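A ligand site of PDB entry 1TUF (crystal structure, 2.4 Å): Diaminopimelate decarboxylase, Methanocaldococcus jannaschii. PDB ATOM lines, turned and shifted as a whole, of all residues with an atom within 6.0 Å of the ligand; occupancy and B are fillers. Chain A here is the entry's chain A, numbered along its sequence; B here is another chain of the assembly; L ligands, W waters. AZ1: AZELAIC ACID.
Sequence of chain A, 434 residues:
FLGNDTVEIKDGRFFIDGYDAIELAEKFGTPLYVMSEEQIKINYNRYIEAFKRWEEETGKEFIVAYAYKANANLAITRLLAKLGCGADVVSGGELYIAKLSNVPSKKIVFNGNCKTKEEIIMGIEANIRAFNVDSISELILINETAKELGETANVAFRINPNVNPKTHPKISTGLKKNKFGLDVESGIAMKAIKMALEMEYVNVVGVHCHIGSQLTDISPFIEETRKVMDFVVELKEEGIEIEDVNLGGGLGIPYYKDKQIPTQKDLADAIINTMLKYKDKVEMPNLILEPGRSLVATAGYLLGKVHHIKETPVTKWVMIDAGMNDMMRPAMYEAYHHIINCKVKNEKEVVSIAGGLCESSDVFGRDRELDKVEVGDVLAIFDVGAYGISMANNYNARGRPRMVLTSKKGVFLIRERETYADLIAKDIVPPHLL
LLP 69 touches the ligand (O3 to OXT2, 3.7 Å).
His 210 touches the ligand (CE1 to O2, 3.6 Å).
Gly 212 touches the ligand (CA to O2, 3.7 Å).
OG of Ser 213 touches C5 of the ligand, 3.6 Å away.
Tyr 333 touches the ligand.
Tyr 387 touches the ligand.
Cys 358 of chain B touches the ligand.
Glu 359 of chain B touches the ligand (OE2 to C7, 3.0 Å).
Ser 360 of chain B touches the ligand (OG to C8, 3.6 Å).
Tyr 395 of chain B touches the ligand (OH to C4, 3.6 Å).
Hydrophobic or aromatic side chains within 4 Å of the ligand: His 210, Tyr 333 and Tyr 387.
Within 4 Å of the ligand: LLP 69, His 210, Gly 212, Ser 213, Arg 293, Arg 329, Tyr 333, Tyr 387, Cys 358 of chain B, Glu 359 of chain B, Ser 360 of chain B and Tyr 395 of chain B.
The nearest printed residue that does not touch the ligand is Met 391 (4.4 Å).
Water W3 bridges OXT of the ligand (2.7 Å) and NH2 of Arg 329 (3.4 Å).
Water W2 lies within hydrogen-bond range of the side-chain carboxylate (OE2) of Glu 359 of chain B (2.5 Å), the side-chain hydroxyl (OG) of Ser 360 of chain B (2.9 Å) and the backbone NH (N) of Ser 361 of chain B (2.9 Å).
Water W1 lies within hydrogen-bond range of O3 of LLP 69, NH2 of Arg 158, OXT2 of the ligand and SG of Cys 358 of chain B.
NE of Arg 329 lies within salt-bridge range of OXT of the ligand (2.6 Å).
NH1 of Arg 293 is in salt-bridge range of OXT of the ligand.
OP2 of LLP 69 is in hydrogen-bond range of the side-chain hydroxyl (OH) of Tyr 387 (2.7 Å).
The guanidinium group (NH1) of Arg 293 is in hydrogen-bond range of the side-chain hydroxyl (OH) of Tyr 255.
OG of Ser 213 lies within hydrogen-bond range of OP1 of LLP 69.
NH2 of Arg 293 sits at hydrogen-bond distance from OG of Ser 213 (2.7 Å).
The side-chain carboxylate of Glu 359 of chain B lies within hydrogen-bond range of the side-chain hydroxyl of Tyr 395 of chain B (2.8 Å).
NE of Arg 293 sits close to OE1 of Gln 214.
The side-chain hydroxyl (OH) of Tyr 255 sits at hydrogen-bond distance from the guanidinium group (NE) of Arg 329, at 3.5 Å.
The backbone NH (N) of Arg 293 sits at hydrogen-bond distance from OP2 of LLP 69, at 2.6 Å.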
ATOM      1  N1  LLP A  69      29.131  12.591 -17.645  1.00  0.00           N
ATOM      2  C2  LLP A  69      28.906  11.305 -18.155  1.00  0.00           C
ATOM      3  C2' LLP A  69      30.117  10.671 -18.813  1.00  0.00           C
ATOM      4  C3  LLP A  69      27.598  10.738 -18.018  1.00  0.00           C
ATOM      5  O3  LLP A  69      27.415   9.474 -18.525  1.00  0.00           O
ATOM      6  C4  LLP A  69      26.539  11.434 -17.376  1.00  0.00           C
ATOM      7  C4' LLP A  69      25.118  10.776 -17.245  1.00  0.00           C
ATOM      8  C5  LLP A  69      26.792  12.784 -16.850  1.00  0.00           C
ATOM      9  C6  LLP A  69      28.096  13.277 -17.022  1.00  0.00           C
ATOM     10  C5' LLP A  69      25.845  13.706 -16.131  1.00  0.00           C
ATOM     11  OP4 LLP A  69      25.124  13.179 -15.071  1.00  0.00           O
ATOM     12  P   LLP A  69      24.304  14.057 -14.102  1.00  0.00           P
ATOM     13  OP1 LLP A  69      23.738  13.046 -13.181  1.00  0.00           O
ATOM     14  OP2 LLP A  69      23.264  14.749 -14.899  1.00  0.00           O
ATOM     15  OP3 LLP A  69      25.166  14.991 -13.402  1.00  0.00           O
ATOM     16  N   LLP A  69      22.799  15.313 -22.449  1.00  0.00           N
ATOM     17  CA  LLP A  69      21.775  14.285 -22.339  1.00  0.00           C
ATOM     18  CB  LLP A  69      22.385  12.906 -22.067  1.00  0.00           C
ATOM     19  CG  LLP A  69      23.216  12.798 -20.799  1.00  0.00           C
ATOM     20  CD  LLP A  69      23.763  11.372 -20.652  1.00  0.00           C
ATOM     21  CE  LLP A  69      23.461  10.722 -19.298  1.00  0.00           C
ATOM     22  NZ  LLP A  69      24.697  10.485 -18.517  1.00  0.00           N
ATOM     23  C   LLP A  69      20.704  14.597 -21.293  1.00  0.00           C
ATOM     24  O   LLP A  69      19.630  13.997 -21.300  1.00  0.00           O
ATOM     25  N   ARG A 158      38.914   7.987 -20.241  1.00  0.00           N
ATOM     26  CA  ARG A 158      37.946   7.651 -19.213  1.00  0.00           C
ATOM     27  C   ARG A 158      38.522   6.417 -18.543  1.00  0.00           C
ATOM     28  O   ARG A 158      38.694   5.365 -19.168  1.00  0.00           O
ATOM     29  CB  ARG A 158      36.564   7.368 -19.799  1.00  0.00           C
ATOM     30  CG  ARG A 158      35.503   7.067 -18.754  1.00  0.00           C
ATOM     31  CD  ARG A 158      34.096   6.970 -19.341  1.00  0.00           C
ATOM     32  NE  ARG A 158      33.096   6.736 -18.284  1.00  0.00           N
ATOM     33  CZ  ARG A 158      31.780   6.914 -18.421  1.00  0.00           C
ATOM     34  NH1 ARG A 158      31.273   7.323 -19.572  1.00  0.00           N
ATOM     35  NH2 ARG A 158      30.979   6.670 -17.387  1.00  0.00           N
ATOM     36  N   PHE A 180      31.728   1.167 -19.585  1.00  0.00           N
ATOM     37  CA  PHE A 180      32.599   2.340 -19.711  1.00  0.00           C
ATOM     38  C   PHE A 180      34.028   2.188 -19.194  1.00  0.00           C
ATOM     39  O   PHE A 180      34.382   1.210 -18.554  1.00  0.00           O
ATOM     40  CB  PHE A 180      31.973   3.514 -18.973  1.00  0.00           C
ATOM     41  CG  PHE A 180      30.540   3.729 -19.290  1.00  0.00           C
ATOM     42  CD1 PHE A 180      30.159   4.199 -20.540  1.00  0.00           C
ATOM     43  CD2 PHE A 180      29.551   3.488 -18.343  1.00  0.00           C
ATOM     44  CE1 PHE A 180      28.829   4.418 -20.843  1.00  0.00           C
ATOM     45  CE2 PHE A 180      28.213   3.710 -18.630  1.00  0.00           C
ATOM     46  CZ  PHE A 180      27.852   4.179 -19.891  1.00  0.00           C
ATOM     47  N   HIS A 210      33.715   9.221 -14.527  1.00  0.00           N
ATOM     48  CA  HIS A 210      32.338   9.518 -14.120  1.00  0.00           C
ATOM     49  C   HIS A 210      31.877   8.317 -13.289  1.00  0.00           C
ATOM     50  O   HIS A 210      31.786   7.206 -13.802  1.00  0.00           O
ATOM     51  CB  HIS A 210      31.436   9.706 -15.349  1.00  0.00           C
ATOM     52  CG  HIS A 210      30.011  10.047 -14.996  1.00  0.00           C
ATOM     53  ND1 HIS A 210      28.983   9.142 -15.110  1.00  0.00           N
ATOM     54  CD2 HIS A 210      29.471  11.179 -14.475  1.00  0.00           C
ATOM     55  CE1 HIS A 210      27.864   9.693 -14.666  1.00  0.00           C
ATOM     56  NE2 HIS A 210      28.134  10.927 -14.275  1.00  0.00           N
ATOM     57  N   ILE A 211      31.590   8.576 -12.011  1.00  0.00           N
ATOM     58  CA  ILE A 211      31.194   7.535 -11.052  1.00  0.00           C
ATOM     59  C   ILE A 211      29.714   7.240 -10.829  1.00  0.00           C
ATOM     60  O   ILE A 211      29.375   6.240 -10.184  1.00  0.00           O
ATOM     61  CB  ILE A 211      31.761   7.832  -9.651  1.00  0.00           C
ATOM     62  CG1 ILE A 211      31.221   9.170  -9.147  1.00  0.00           C
ATOM     63  CG2 ILE A 211      33.273   7.788  -9.681  1.00  0.00           C
ATOM     64  CD1 ILE A 211      31.515   9.459  -7.670  1.00  0.00           C
ATOM     65  N   GLY A 212      28.829   8.096 -11.310  1.00  0.00           N
ATOM     66  CA  GLY A 212      27.420   7.818 -11.095  1.00  0.00           C
ATOM     67  C   GLY A 212      26.528   9.030 -11.240  1.00  0.00           C
ATOM     68  O   GLY A 212      26.950  10.068 -11.750  1.00  0.00           O
ATOM     69  N   SER A 213      25.297   8.894 -10.772  1.00  0.00           N
ATOM     70  CA  SER A 213      24.330   9.974 -10.869  1.00  0.00           C
ATOM     71  C   SER A 213      23.414   9.999  -9.664  1.00  0.00           C
ATOM     72  O   SER A 213      23.186   8.970  -9.009  1.00  0.00           O
ATOM     73  CB  SER A 213      23.507   9.836 -12.161  1.00  0.00           C
ATOM     74  OG  SER A 213      22.529  10.852 -12.240  1.00  0.00           O
ATOM     75  N   GLN A 214      22.897  11.192  -9.385  1.00  0.00           N
ATOM     76  CA  GLN A 214      22.026  11.445  -8.252  1.00  0.00           C
ATOM     77  C   GLN A 214      22.670  11.029  -6.927  1.00  0.00           C
ATOM     78  O   GLN A 214      22.009  10.506  -6.026  1.00  0.00           O
ATOM     79  CB  GLN A 214      20.686  10.728  -8.447  1.00  0.00           C
ATOM     80  CG  GLN A 214      19.630  11.073  -7.393  1.00  0.00           C
ATOM     81  CD  GLN A 214      19.467  12.569  -7.194  1.00  0.00           C
ATOM     82  OE1 GLN A 214      19.721  13.360  -8.098  1.00  0.00           O
ATOM     83  NE2 GLN A 214      19.012  12.967  -6.000  1.00  0.00           N
ATOM     84  N   TYR A 255      15.215  16.377  -4.867  1.00  0.00           N
ATOM     85  CA  TYR A 255      13.901  15.839  -5.249  1.00  0.00           C
ATOM     86  C   TYR A 255      13.013  15.806  -4.011  1.00  0.00           C
ATOM     87  O   TYR A 255      11.857  16.236  -4.047  1.00  0.00           O
ATOM     88  CB  TYR A 255      14.015  14.429  -5.842  1.00  0.00           C
ATOM     89  CG  TYR A 255      14.520  14.408  -7.273  1.00  0.00           C
ATOM     90  CD1 TYR A 255      13.831  15.068  -8.289  1.00  0.00           C
ATOM     91  CD2 TYR A 255      15.707  13.750  -7.593  1.00  0.00           C
ATOM     92  CE1 TYR A 255      14.313  15.075  -9.607  1.00  0.00           C
ATOM     93  CE2 TYR A 255      16.189  13.748  -8.890  1.00  0.00           C
ATOM     94  CZ  TYR A 255      15.503  14.407  -9.892  1.00  0.00           C
ATOM     95  OH  TYR A 255      16.036  14.437 -11.158  1.00  0.00           O
ATOM     96  N   ARG A 293      21.983  16.980 -14.283  1.00  0.00           N
ATOM     97  CA  ARG A 293      20.825  17.159 -13.431  1.00  0.00           C
ATOM     98  C   ARG A 293      21.015  18.352 -12.494  1.00  0.00           C
ATOM     99  O   ARG A 293      20.082  19.094 -12.217  1.00  0.00           O
ATOM    100  CB  ARG A 293      20.614  15.882 -12.622  1.00  0.00           C
ATOM    101  CG  ARG A 293      19.287  15.789 -11.878  1.00  0.00           C
ATOM    102  CD  ARG A 293      19.381  14.717 -10.793  1.00  0.00           C
ATOM    103  NE  ARG A 293      19.940  13.462 -11.306  1.00  0.00           N
ATOM    104  CZ  ARG A 293      19.280  12.602 -12.072  1.00  0.00           C
ATOM    105  NH1 ARG A 293      18.023  12.862 -12.418  1.00  0.00           N
ATOM    106  NH2 ARG A 293      19.867  11.485 -12.491  1.00  0.00           N
ATOM    107  N   ARG A 329      10.582   9.685 -15.965  1.00  0.00           N
ATOM    108  CA  ARG A 329      11.189   9.383 -14.675  1.00  0.00           C
ATOM    109  C   ARG A 329      10.358   8.544 -13.663  1.00  0.00           C
ATOM    110  O   ARG A 329      10.803   7.476 -13.232  1.00  0.00           O
ATOM    111  CB  ARG A 329      11.702  10.680 -14.041  1.00  0.00           C
ATOM    112  CG  ARG A 329      12.609  10.468 -12.850  1.00  0.00           C
ATOM    113  CD  ARG A 329      13.466  11.708 -12.537  1.00  0.00           C
ATOM    114  NE  ARG A 329      14.450  11.380 -11.512  1.00  0.00           N
ATOM    115  CZ  ARG A 329      14.175  11.321 -10.200  1.00  0.00           C
ATOM    116  NH1 ARG A 329      12.953  11.586  -9.761  1.00  0.00           N
ATOM    117  NH2 ARG A 329      15.119  10.947  -9.353  1.00  0.00           N
ATOM    118  N   TYR A 333      11.666   4.562 -13.061  1.00  0.00           N
ATOM    119  CA  TYR A 333      12.465   4.272 -11.876  1.00  0.00           C
ATOM    120  C   TYR A 333      11.671   4.313 -10.580  1.00  0.00           C
ATOM    121  O   TYR A 333      12.198   3.998  -9.517  1.00  0.00           O
ATOM    122  CB  TYR A 333      13.616   5.280 -11.785  1.00  0.00           C
ATOM    123  CG  TYR A 333      14.413   5.466 -13.075  1.00  0.00           C
ATOM    124  CD1 TYR A 333      15.416   4.555 -13.441  1.00  0.00           C
ATOM    125  CD2 TYR A 333      14.189   6.558 -13.902  1.00  0.00           C
ATOM    126  CE1 TYR A 333      16.182   4.740 -14.605  1.00  0.00           C
ATOM    127  CE2 TYR A 333      14.935   6.751 -15.062  1.00  0.00           C
ATOM    128  CZ  TYR A 333      15.932   5.842 -15.413  1.00  0.00           C
ATOM    129  OH  TYR A 333      16.664   6.049 -16.562  1.00  0.00           O
ATOM    130  N   ALA A 335      10.869   6.840  -9.282  1.00  0.00           N
ATOM    131  CA  ALA A 335      11.524   7.949  -8.607  1.00  0.00           C
ATOM    132  C   ALA A 335      10.530   8.988  -8.100  1.00  0.00           C
ATOM    133  O   ALA A 335       9.418   9.122  -8.637  1.00  0.00           O
ATOM    134  CB  ALA A 335      12.542   8.590  -9.535  1.00  0.00           C
ATOM    135  N   TYR A 387      16.415  15.164 -17.711  1.00  0.00           N
ATOM    136  CA  TYR A 387      15.899  13.849 -18.023  1.00  0.00           C
ATOM    137  C   TYR A 387      14.368  13.841 -18.038  1.00  0.00           C
ATOM    138  O   TYR A 387      13.745  12.893 -17.569  1.00  0.00           O
ATOM    139  CB  TYR A 387      16.443  12.843 -16.997  1.00  0.00           C
ATOM    140  CG  TYR A 387      17.956  12.878 -16.898  1.00  0.00           C
ATOM    141  CD1 TYR A 387      18.752  12.424 -17.953  1.00  0.00           C
ATOM    142  CD2 TYR A 387      18.583  13.435 -15.783  1.00  0.00           C
ATOM    143  CE1 TYR A 387      20.148  12.514 -17.896  1.00  0.00           C
ATOM    144  CE2 TYR A 387      19.981  13.524 -15.712  1.00  0.00           C
ATOM    145  CZ  TYR A 387      20.742  13.069 -16.776  1.00  0.00           C
ATOM    146  OH  TYR A 387      22.114  13.184 -16.728  1.00  0.00           O
ATOM    147  N   MET A 391      13.927  12.484 -22.520  1.00  0.00           N
ATOM    148  CA  MET A 391      13.579  11.064 -22.580  1.00  0.00           C
ATOM    149  C   MET A 391      12.115  10.875 -22.980  1.00  0.00           C
ATOM    150  O   MET A 391      11.595   9.770 -22.921  1.00  0.00           O
ATOM    151  CB  MET A 391      13.825  10.393 -21.221  1.00  0.00           C
ATOM    152  CG  MET A 391      15.256  10.515 -20.736  1.00  0.00           C
ATOM    153  SD  MET A 391      15.671   9.271 -19.491  1.00  0.00           S
ATOM    154  CE  MET A 391      14.432   9.611 -18.175  1.00  0.00           C
ATOM    155  N   CYS B 358      25.301   6.801 -23.209  1.00  0.00           N
ATOM    156  CA  CYS B 358      26.024   6.888 -21.935  1.00  0.00           C
ATOM    157  C   CYS B 358      25.030   6.718 -20.809  1.00  0.00           C
ATOM    158  O   CYS B 358      24.594   7.684 -20.189  1.00  0.00           O
ATOM    159  CB  CYS B 358      26.749   8.232 -21.794  1.00  0.00           C
ATOM    160  SG  CYS B 358      28.530   8.108 -22.157  1.00  0.00           S
ATOM    161  N   GLU B 359      24.665   5.462 -20.593  1.00  0.00           N
ATOM    162  CA  GLU B 359      23.725   5.107 -19.549  1.00  0.00           C
ATOM    163  C   GLU B 359      24.059   3.654 -19.259  1.00  0.00           C
ATOM    164  O   GLU B 359      23.952   2.814 -20.139  1.00  0.00           O
ATOM    165  CB  GLU B 359      22.309   5.247 -20.091  1.00  0.00           C
ATOM    166  CG  GLU B 359      21.213   5.060 -19.066  1.00  0.00           C
ATOM    167  CD  GLU B 359      21.172   6.174 -18.031  1.00  0.00           C
ATOM    168  OE1 GLU B 359      21.431   7.340 -18.398  1.00  0.00           O
ATOM    169  OE2 GLU B 359      20.846   5.882 -16.863  1.00  0.00           O
ATOM    170  N   SER B 360      24.496   3.369 -18.036  1.00  0.00           N
ATOM    171  CA  SER B 360      24.879   2.009 -17.679  1.00  0.00           C
ATOM    172  C   SER B 360      23.822   0.964 -18.010  1.00  0.00           C
ATOM    173  O   SER B 360      24.151  -0.169 -18.314  1.00  0.00           O
ATOM    174  CB  SER B 360      25.240   1.935 -16.189  1.00  0.00           C
ATOM    175  OG  SER B 360      24.210   2.452 -15.360  1.00  0.00           O
ATOM    176  N   SER B 361      22.546   1.347 -17.947  1.00  0.00           N
ATOM    177  CA  SER B 361      21.467   0.423 -18.242  1.00  0.00           C
ATOM    178  C   SER B 361      21.378   0.107 -19.729  1.00  0.00           C
ATOM    179  O   SER B 361      20.702  -0.851 -20.129  1.00  0.00           O
ATOM    180  CB  SER B 361      20.132   0.982 -17.738  1.00  0.00           C
ATOM    181  OG  SER B 361      19.806   2.186 -18.411  1.00  0.00           O
ATOM    182  N   TYR B 395      16.778   9.929 -26.688  1.00  0.00           N
ATOM    183  CA  TYR B 395      17.718  10.065 -25.578  1.00  0.00           C
ATOM    184  C   TYR B 395      19.138  10.136 -26.129  1.00  0.00           C
ATOM    185  O   TYR B 395      19.494   9.410 -27.045  1.00  0.00           O
ATOM    186  CB  TYR B 395      17.579   8.876 -24.627  1.00  0.00           C
ATOM    187  CG  TYR B 395      18.302   9.061 -23.323  1.00  0.00           C
ATOM    188  CD1 TYR B 395      18.274  10.297 -22.659  1.00  0.00           C
ATOM    189  CD2 TYR B 395      18.979   8.001 -22.709  1.00  0.00           C
ATOM    190  CE1 TYR B 395      18.892  10.473 -21.434  1.00  0.00           C
ATOM    191  CE2 TYR B 395      19.605   8.166 -21.479  1.00  0.00           C
ATOM    192  CZ  TYR B 395      19.560   9.403 -20.848  1.00  0.00           C
ATOM    193  OH  TYR B 395      20.138   9.556 -19.612  1.00  0.00           O
HETATM  194  C   AZ1 L   1      16.574   9.727 -13.402  1.00  0.00           C
HETATM  195  C2  AZ1 L   1      17.818   9.491 -14.265  1.00  0.00           C
HETATM  196  C3  AZ1 L   1      18.452   9.088 -15.600  1.00  0.00           C
HETATM  197  C4  AZ1 L   1      19.911   8.988 -16.044  1.00  0.00           C
HETATM  198  C5  AZ1 L   1      21.121   9.145 -15.115  1.00  0.00           C
HETATM  199  C6  AZ1 L   1      22.338   8.284 -15.436  1.00  0.00           C
HETATM  200  C7  AZ1 L   1      22.800   6.953 -14.823  1.00  0.00           C
HETATM  201  C8  AZ1 L   1      23.835   6.031 -15.475  1.00  0.00           C
HETATM  202  C9  AZ1 L   1      25.268   6.543 -15.464  1.00  0.00           C
HETATM  203  OXT AZ1 L   1      16.672  10.130 -12.116  1.00  0.00           O
HETATM  204  O   AZ1 L   1      15.460   9.555 -13.895  1.00  0.00           O
HETATM  205  O2  AZ1 L   1      25.893   6.716 -14.254  1.00  0.00           O
HETATM  206 OXT2 AZ1 L   1      25.789   6.800 -16.563  1.00  0.00           O
HETATM  207  O   HOH W   1      28.500   7.129 -18.656  1.00  0.00           O
HETATM  208  O   HOH W   2      21.696   3.589 -16.238  1.00  0.00           O
HETATM  209  O   HOH W   3      17.576   8.648 -10.060  1.00  0.00           O
